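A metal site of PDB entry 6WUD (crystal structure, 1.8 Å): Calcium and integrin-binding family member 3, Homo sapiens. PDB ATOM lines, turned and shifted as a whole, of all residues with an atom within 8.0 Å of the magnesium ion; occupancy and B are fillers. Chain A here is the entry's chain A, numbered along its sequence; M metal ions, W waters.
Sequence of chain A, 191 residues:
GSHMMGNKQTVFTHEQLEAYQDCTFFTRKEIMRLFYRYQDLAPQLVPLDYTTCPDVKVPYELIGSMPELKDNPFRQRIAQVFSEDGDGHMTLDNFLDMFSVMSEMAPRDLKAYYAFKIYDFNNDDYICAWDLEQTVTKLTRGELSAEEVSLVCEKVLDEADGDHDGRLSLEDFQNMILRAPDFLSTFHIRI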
ATOM      1  N   ARG A  77      29.944  11.598   7.219  1.00  0.00           N
ATOM      2  CA  ARG A  77      29.971  10.275   7.848  1.00  0.00           C
ATOM      3  C   ARG A  77      30.783   9.253   7.038  1.00  0.00           C
ATOM      4  O   ARG A  77      31.468   8.403   7.616  1.00  0.00           O
ATOM      5  CB  ARG A  77      28.555   9.703   8.031  1.00  0.00           C
ATOM      6  CG  ARG A  77      27.735  10.288   9.106  1.00  0.00           C
ATOM      7  CD  ARG A  77      28.322  10.026  10.467  1.00  0.00           C
ATOM      8  NE  ARG A  77      28.485   8.609  10.732  1.00  0.00           N
ATOM      9  CZ  ARG A  77      29.412   8.103  11.528  1.00  0.00           C
ATOM     10  NH1 ARG A  77      30.276   8.910  12.160  1.00  0.00           N
ATOM     11  NH2 ARG A  77      29.484   6.799  11.713  1.00  0.00           N
ATOM     12  N   PHE A 116      25.971   0.148   7.630  1.00  0.00           N
ATOM     13  CA  PHE A 116      25.642   0.137   9.055  1.00  0.00           C
ATOM     14  C   PHE A 116      26.510   1.119   9.831  1.00  0.00           C
ATOM     15  O   PHE A 116      26.006   1.863  10.688  1.00  0.00           O
ATOM     16  CB  PHE A 116      25.797  -1.290   9.596  1.00  0.00           C
ATOM     17  CG  PHE A 116      25.449  -1.428  11.053  1.00  0.00           C
ATOM     18  CD1 PHE A 116      24.126  -1.388  11.447  1.00  0.00           C
ATOM     19  CD2 PHE A 116      26.435  -1.618  12.007  1.00  0.00           C
ATOM     20  CE1 PHE A 116      23.789  -1.508  12.771  1.00  0.00           C
ATOM     21  CE2 PHE A 116      26.099  -1.738  13.331  1.00  0.00           C
ATOM     22  CZ  PHE A 116      24.779  -1.689  13.714  1.00  0.00           C
ATOM     23  N   LYS A 117      27.809   1.124   9.560  1.00  0.00           N
ATOM     24  CA  LYS A 117      28.729   2.024  10.243  1.00  0.00           C
ATOM     25  C   LYS A 117      28.429   3.473   9.919  1.00  0.00           C
ATOM     26  O   LYS A 117      28.492   4.346  10.789  1.00  0.00           O
ATOM     27  CB  LYS A 117      30.178   1.678   9.835  1.00  0.00           C
ATOM     28  CG  LYS A 117      30.781   0.466  10.563  1.00  0.00           C
ATOM     29  CD  LYS A 117      30.728   0.667  12.084  1.00  0.00           C
ATOM     30  CE  LYS A 117      31.707  -0.250  12.835  1.00  0.00           C
ATOM     31  NZ  LYS A 117      32.195  -1.404  12.003  1.00  0.00           N
ATOM     32  N   TYR A 119      25.541   4.881   9.130  1.00  0.00           N
ATOM     33  CA  TYR A 119      24.298   5.360   9.722  1.00  0.00           C
ATOM     34  C   TYR A 119      24.290   5.207  11.251  1.00  0.00           C
ATOM     35  O   TYR A 119      23.375   5.736  11.897  1.00  0.00           O
ATOM     36  CB  TYR A 119      23.113   4.637   9.064  1.00  0.00           C
ATOM     37  CG  TYR A 119      23.056   4.923   7.559  1.00  0.00           C
ATOM     38  CD1 TYR A 119      23.045   6.222   7.079  1.00  0.00           C
ATOM     39  CD2 TYR A 119      23.071   3.902   6.638  1.00  0.00           C
ATOM     40  CE1 TYR A 119      23.039   6.482   5.698  1.00  0.00           C
ATOM     41  CE2 TYR A 119      23.055   4.153   5.246  1.00  0.00           C
ATOM     42  CZ  TYR A 119      23.025   5.437   4.785  1.00  0.00           C
ATOM     43  OH  TYR A 119      22.998   5.715   3.429  1.00  0.00           O
ATOM     44  N   ASP A 120      25.313   4.566  11.825  1.00  0.00           N
ATOM     45  CA  ASP A 120      25.470   4.510  13.280  1.00  0.00           C
ATOM     46  C   ASP A 120      26.223   5.778  13.696  1.00  0.00           C
ATOM     47  O   ASP A 120      27.438   5.771  13.974  1.00  0.00           O
ATOM     48  CB  ASP A 120      26.163   3.230  13.695  1.00  0.00           C
ATOM     49  CG  ASP A 120      26.618   3.259  15.142  1.00  0.00           C
ATOM     50  OD1 ASP A 120      26.055   4.016  15.946  1.00  0.00           O
ATOM     51  OD2 ASP A 120      27.556   2.489  15.460  1.00  0.00           O
ATOM     52  N   PHE A 121      25.485   6.883  13.743  1.00  0.00           N
ATOM     53  CA  PHE A 121      26.090   8.206  13.922  1.00  0.00           C
ATOM     54  C   PHE A 121      26.840   8.303  15.250  1.00  0.00           C
ATOM     55  O   PHE A 121      27.885   8.950  15.319  1.00  0.00           O
ATOM     56  CB  PHE A 121      25.025   9.297  13.851  1.00  0.00           C
ATOM     57  CG  PHE A 121      24.671   9.743  12.448  1.00  0.00           C
ATOM     58  CD1 PHE A 121      25.207  10.922  11.926  1.00  0.00           C
ATOM     59  CD2 PHE A 121      23.801   9.000  11.674  1.00  0.00           C
ATOM     60  CE1 PHE A 121      24.896  11.332  10.627  1.00  0.00           C
ATOM     61  CE2 PHE A 121      23.479   9.391  10.355  1.00  0.00           C
ATOM     62  CZ  PHE A 121      24.030  10.545   9.828  1.00  0.00           C
ATOM     63  N   ASN A 122      26.351   7.655  16.301  1.00  0.00           N
ATOM     64  CA  ASN A 122      26.986   7.740  17.610  1.00  0.00           C
ATOM     65  C   ASN A 122      28.013   6.639  17.849  1.00  0.00           C
ATOM     66  O   ASN A 122      28.533   6.523  18.957  1.00  0.00           O
ATOM     67  CB  ASN A 122      25.942   7.745  18.743  1.00  0.00           C
ATOM     68  CG  ASN A 122      24.990   6.547  18.713  1.00  0.00           C
ATOM     69  OD1 ASN A 122      25.215   5.539  18.063  1.00  0.00           O
ATOM     70  ND2 ASN A 122      23.896   6.664  19.466  1.00  0.00           N
ATOM     71  N   ASN A 123      28.329   5.851  16.832  1.00  0.00           N
ATOM     72  CA  ASN A 123      29.462   4.916  16.866  1.00  0.00           C
ATOM     73  C   ASN A 123      29.393   3.968  18.067  1.00  0.00           C
ATOM     74  O   ASN A 123      30.406   3.677  18.710  1.00  0.00           O
ATOM     75  CB  ASN A 123      30.787   5.690  16.858  1.00  0.00           C
ATOM     76  CG  ASN A 123      30.833   6.800  15.817  1.00  0.00           C
ATOM     77  OD1 ASN A 123      30.803   6.529  14.616  1.00  0.00           O
ATOM     78  ND2 ASN A 123      30.901   8.058  16.275  1.00  0.00           N
ATOM     79  N   ASP A 124      28.218   3.421  18.341  1.00  0.00           N
ATOM     80  CA  ASP A 124      28.075   2.488  19.457  1.00  0.00           C
ATOM     81  C   ASP A 124      27.742   1.062  19.001  1.00  0.00           C
ATOM     82  O   ASP A 124      27.378   0.232  19.841  1.00  0.00           O
ATOM     83  CB  ASP A 124      27.009   2.987  20.437  1.00  0.00           C
ATOM     84  CG  ASP A 124      25.623   3.008  19.840  1.00  0.00           C
ATOM     85  OD1 ASP A 124      25.509   2.912  18.594  1.00  0.00           O
ATOM     86  OD2 ASP A 124      24.641   3.128  20.613  1.00  0.00           O
ATOM     87  N   ASP A 125      27.892   0.767  17.713  1.00  0.00           N
ATOM     88  CA  ASP A 125      27.644  -0.536  17.105  1.00  0.00           C
ATOM     89  C   ASP A 125      26.157  -0.876  17.054  1.00  0.00           C
ATOM     90  O   ASP A 125      25.787  -2.043  16.899  1.00  0.00           O
ATOM     91  CB  ASP A 125      28.400  -1.656  17.819  1.00  0.00           C
ATOM     92  CG  ASP A 125      29.912  -1.532  17.685  1.00  0.00           C
ATOM     93  OD1 ASP A 125      30.616  -1.915  18.641  1.00  0.00           O
ATOM     94  OD2 ASP A 125      30.404  -1.072  16.635  1.00  0.00           O
ATOM     95  N   TYR A 126      25.298   0.122  17.194  1.00  0.00           N
ATOM     96  CA  TYR A 126      23.859  -0.026  17.099  1.00  0.00           C
ATOM     97  C   TYR A 126      23.298   1.174  16.359  1.00  0.00           C
ATOM     98  O   TYR A 126      23.892   2.251  16.390  1.00  0.00           O
ATOM     99  CB  TYR A 126      23.163  -0.119  18.468  1.00  0.00           C
ATOM    100  CG  TYR A 126      23.488  -1.391  19.195  1.00  0.00           C
ATOM    101  CD1 TYR A 126      22.735  -2.543  18.971  1.00  0.00           C
ATOM    102  CD2 TYR A 126      24.528  -1.443  20.102  1.00  0.00           C
ATOM    103  CE1 TYR A 126      23.022  -3.708  19.607  1.00  0.00           C
ATOM    104  CE2 TYR A 126      24.825  -2.611  20.740  1.00  0.00           C
ATOM    105  CZ  TYR A 126      24.062  -3.741  20.491  1.00  0.00           C
ATOM    106  OH  TYR A 126      24.349  -4.906  21.127  1.00  0.00           O
ATOM    107  N   ILE A 127      22.146   1.004  15.714  1.00  0.00           N
ATOM    108  CA  ILE A 127      21.390   2.124  15.153  1.00  0.00           C
ATOM    109  C   ILE A 127      20.116   2.253  15.975  1.00  0.00           C
ATOM    110  O   ILE A 127      19.222   1.391  15.927  1.00  0.00           O
ATOM    111  CB  ILE A 127      21.082   1.939  13.668  1.00  0.00           C
ATOM    112  CG1 ILE A 127      22.392   2.020  12.880  1.00  0.00           C
ATOM    113  CG2 ILE A 127      20.151   3.037  13.161  1.00  0.00           C
ATOM    114  CD1 ILE A 127      22.223   1.685  11.406  1.00  0.00           C
ATOM    115  N   CYS A 128      20.086   3.293  16.790  1.00  0.00           N
ATOM    116  CA  CYS A 128      18.974   3.580  17.683  1.00  0.00           C
ATOM    117  C   CYS A 128      18.074   4.655  17.102  1.00  0.00           C
ATOM    118  O   CYS A 128      18.287   5.164  15.987  1.00  0.00           O
ATOM    119  CB  CYS A 128      19.533   3.990  19.043  1.00  0.00           C
ATOM    120  SG  CYS A 128      20.422   5.543  19.000  1.00  0.00           S
ATOM    121  N   ALA A 129      17.040   5.028  17.877  1.00  0.00           N
ATOM    122  CA  ALA A 129      16.147   6.078  17.433  1.00  0.00           C
ATOM    123  C   ALA A 129      16.878   7.391  17.195  1.00  0.00           C
ATOM    124  O   ALA A 129      16.491   8.160  16.301  1.00  0.00           O
ATOM    125  CB  ALA A 129      15.030   6.294  18.467  1.00  0.00           C
ATOM    126  N   TRP A 130      17.939   7.677  17.964  1.00  0.00           N
ATOM    127  CA  TRP A 130      18.700   8.910  17.741  1.00  0.00           C
ATOM    128  C   TRP A 130      19.517   8.840  16.453  1.00  0.00           C
ATOM    129  O   TRP A 130      19.628   9.829  15.713  1.00  0.00           O
ATOM    130  CB  TRP A 130      19.643   9.182  18.909  1.00  0.00           C
ATOM    131  CG  TRP A 130      20.410  10.471  18.773  1.00  0.00           C
ATOM    132  CD1 TRP A 130      20.023  11.717  19.224  1.00  0.00           C
ATOM    133  CD2 TRP A 130      21.697  10.655  18.173  1.00  0.00           C
ATOM    134  NE1 TRP A 130      20.988  12.650  18.919  1.00  0.00           N
ATOM    135  CE2 TRP A 130      22.023  12.027  18.286  1.00  0.00           C
ATOM    136  CE3 TRP A 130      22.596   9.788  17.544  1.00  0.00           C
ATOM    137  CZ2 TRP A 130      23.206  12.547  17.791  1.00  0.00           C
ATOM    138  CZ3 TRP A 130      23.774  10.300  17.059  1.00  0.00           C
ATOM    139  CH2 TRP A 130      24.068  11.682  17.186  1.00  0.00           C
ATOM    140  N   ASP A 131      20.146   7.697  16.176  1.00  0.00           N
ATOM    141  CA  ASP A 131      20.852   7.546  14.918  1.00  0.00           C
ATOM    142  C   ASP A 131      19.873   7.667  13.749  1.00  0.00           C
ATOM    143  O   ASP A 131      20.193   8.224  12.688  1.00  0.00           O
ATOM    144  CB  ASP A 131      21.548   6.189  14.821  1.00  0.00           C
ATOM    145  CG  ASP A 131      22.768   6.058  15.728  1.00  0.00           C
ATOM    146  OD1 ASP A 131      23.463   7.062  16.000  1.00  0.00           O
ATOM    147  OD2 ASP A 131      23.048   4.909  16.116  1.00  0.00           O
ATOM    148  N   LEU A 132      18.683   7.095  13.911  1.00  0.00           N
ATOM    149  CA  LEU A 132      17.687   7.145  12.839  1.00  0.00           C
ATOM    150  C   LEU A 132      17.214   8.574  12.609  1.00  0.00           C
ATOM    151  O   LEU A 132      16.961   9.000  11.462  1.00  0.00           O
ATOM    152  CB  LEU A 132      16.514   6.230  13.207  1.00  0.00           C
ATOM    153  CG  LEU A 132      16.694   4.726  13.025  1.00  0.00           C
ATOM    154  CD1 LEU A 132      15.463   4.008  13.616  1.00  0.00           C
ATOM    155  CD2 LEU A 132      16.911   4.331  11.597  1.00  0.00           C
ATOM    156  N   ARG A 167      16.564  -1.213  19.151  1.00  0.00           N
ATOM    157  CA  ARG A 167      17.668  -0.661  18.363  1.00  0.00           C
ATOM    158  C   ARG A 167      18.141  -1.736  17.397  1.00  0.00           C
ATOM    159  O   ARG A 167      17.913  -2.916  17.606  1.00  0.00           O
ATOM    160  CB  ARG A 167      18.811  -0.202  19.249  1.00  0.00           C
ATOM    161  CG  ARG A 167      19.396  -1.301  20.053  1.00  0.00           C
ATOM    162  CD  ARG A 167      20.237  -0.784  21.205  1.00  0.00           C
ATOM    163  NE  ARG A 167      20.759  -1.910  21.971  1.00  0.00           N
ATOM    164  CZ  ARG A 167      21.829  -1.864  22.759  1.00  0.00           C
ATOM    165  NH1 ARG A 167      22.526  -0.744  22.906  1.00  0.00           N
ATOM    166  NH2 ARG A 167      22.194  -2.966  23.401  1.00  0.00           N
ATOM    167  N   LEU A 168      18.826  -1.308  16.344  1.00  0.00           N
ATOM    168  CA  LEU A 168      19.230  -2.176  15.259  1.00  0.00           C
ATOM    169  C   LEU A 168      20.675  -2.601  15.483  1.00  0.00           C
ATOM    170  O   LEU A 168      21.587  -1.769  15.457  1.00  0.00           O
ATOM    171  CB  LEU A 168      19.064  -1.498  13.894  1.00  0.00           C
ATOM    172  CG  LEU A 168      17.707  -0.930  13.525  1.00  0.00           C
ATOM    173  CD1 LEU A 168      17.675  -0.396  12.098  1.00  0.00           C
ATOM    174  CD2 LEU A 168      16.569  -1.958  13.739  1.00  0.00           C
HETATM  175 MG    MG M   1      24.411   4.047  17.214  1.00  0.00          MG
HETATM  176  O   HOH W   1      22.878   3.718  18.667  1.00  0.00           O
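The magnesium ion is bound by the side-chain amide oxygen (OD1) of Asn 122 (1.9 Å), the side-chain carboxylate (OD2) of Asp 131 (2.0 Å), the backbone carbonyl oxygen (O) of Tyr 126 (2.0 Å), the side-chain carboxylate (OD1) of Asp 120 (2.1 Å), the side-chain carboxylate (OD1) of Asp 124 (2.1 Å) and water W1 (2.1 Å).
Water W1 lies within hydrogen-bond range of the side-chain carboxylate (OD2) of Asp 124 (2.7 Å), the side-chain sulfur (SG) of Cys 128 (3.1 Å) and the side-chain amide nitrogen (ND2) of Asn 122 (3.2 Å).
Within 4 Å of the magnesium ion: Asp 120, Asn 122, Asp 124, Tyr 126 and Asp 131.
The nearest printed residue that does not touch the magnesium ion is Ile 127 (4.1 Å).
The side-chain carboxylate (OD2) of Asp 120 is in hydrogen-bond range of the backbone NH (N) of Asp 125 (2.9 Å).
NH2 of Arg 77 lies within hydrogen-bond range of O of Asp 120.
ND2 of Asn 122 is in hydrogen-bond range of SG of Cys 128 (3.7 Å).
N of Asp 131 sits at hydrogen-bond distance from SG of Cys 128, at 3.6 Å.
OD1 of Asp 120 sits close to N of Asn 123, 3.1 Å away.
The backbone NH (N) of Phe 121 sits at hydrogen-bond distance from the side-chain carboxylate (OD1) of Asp 131.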
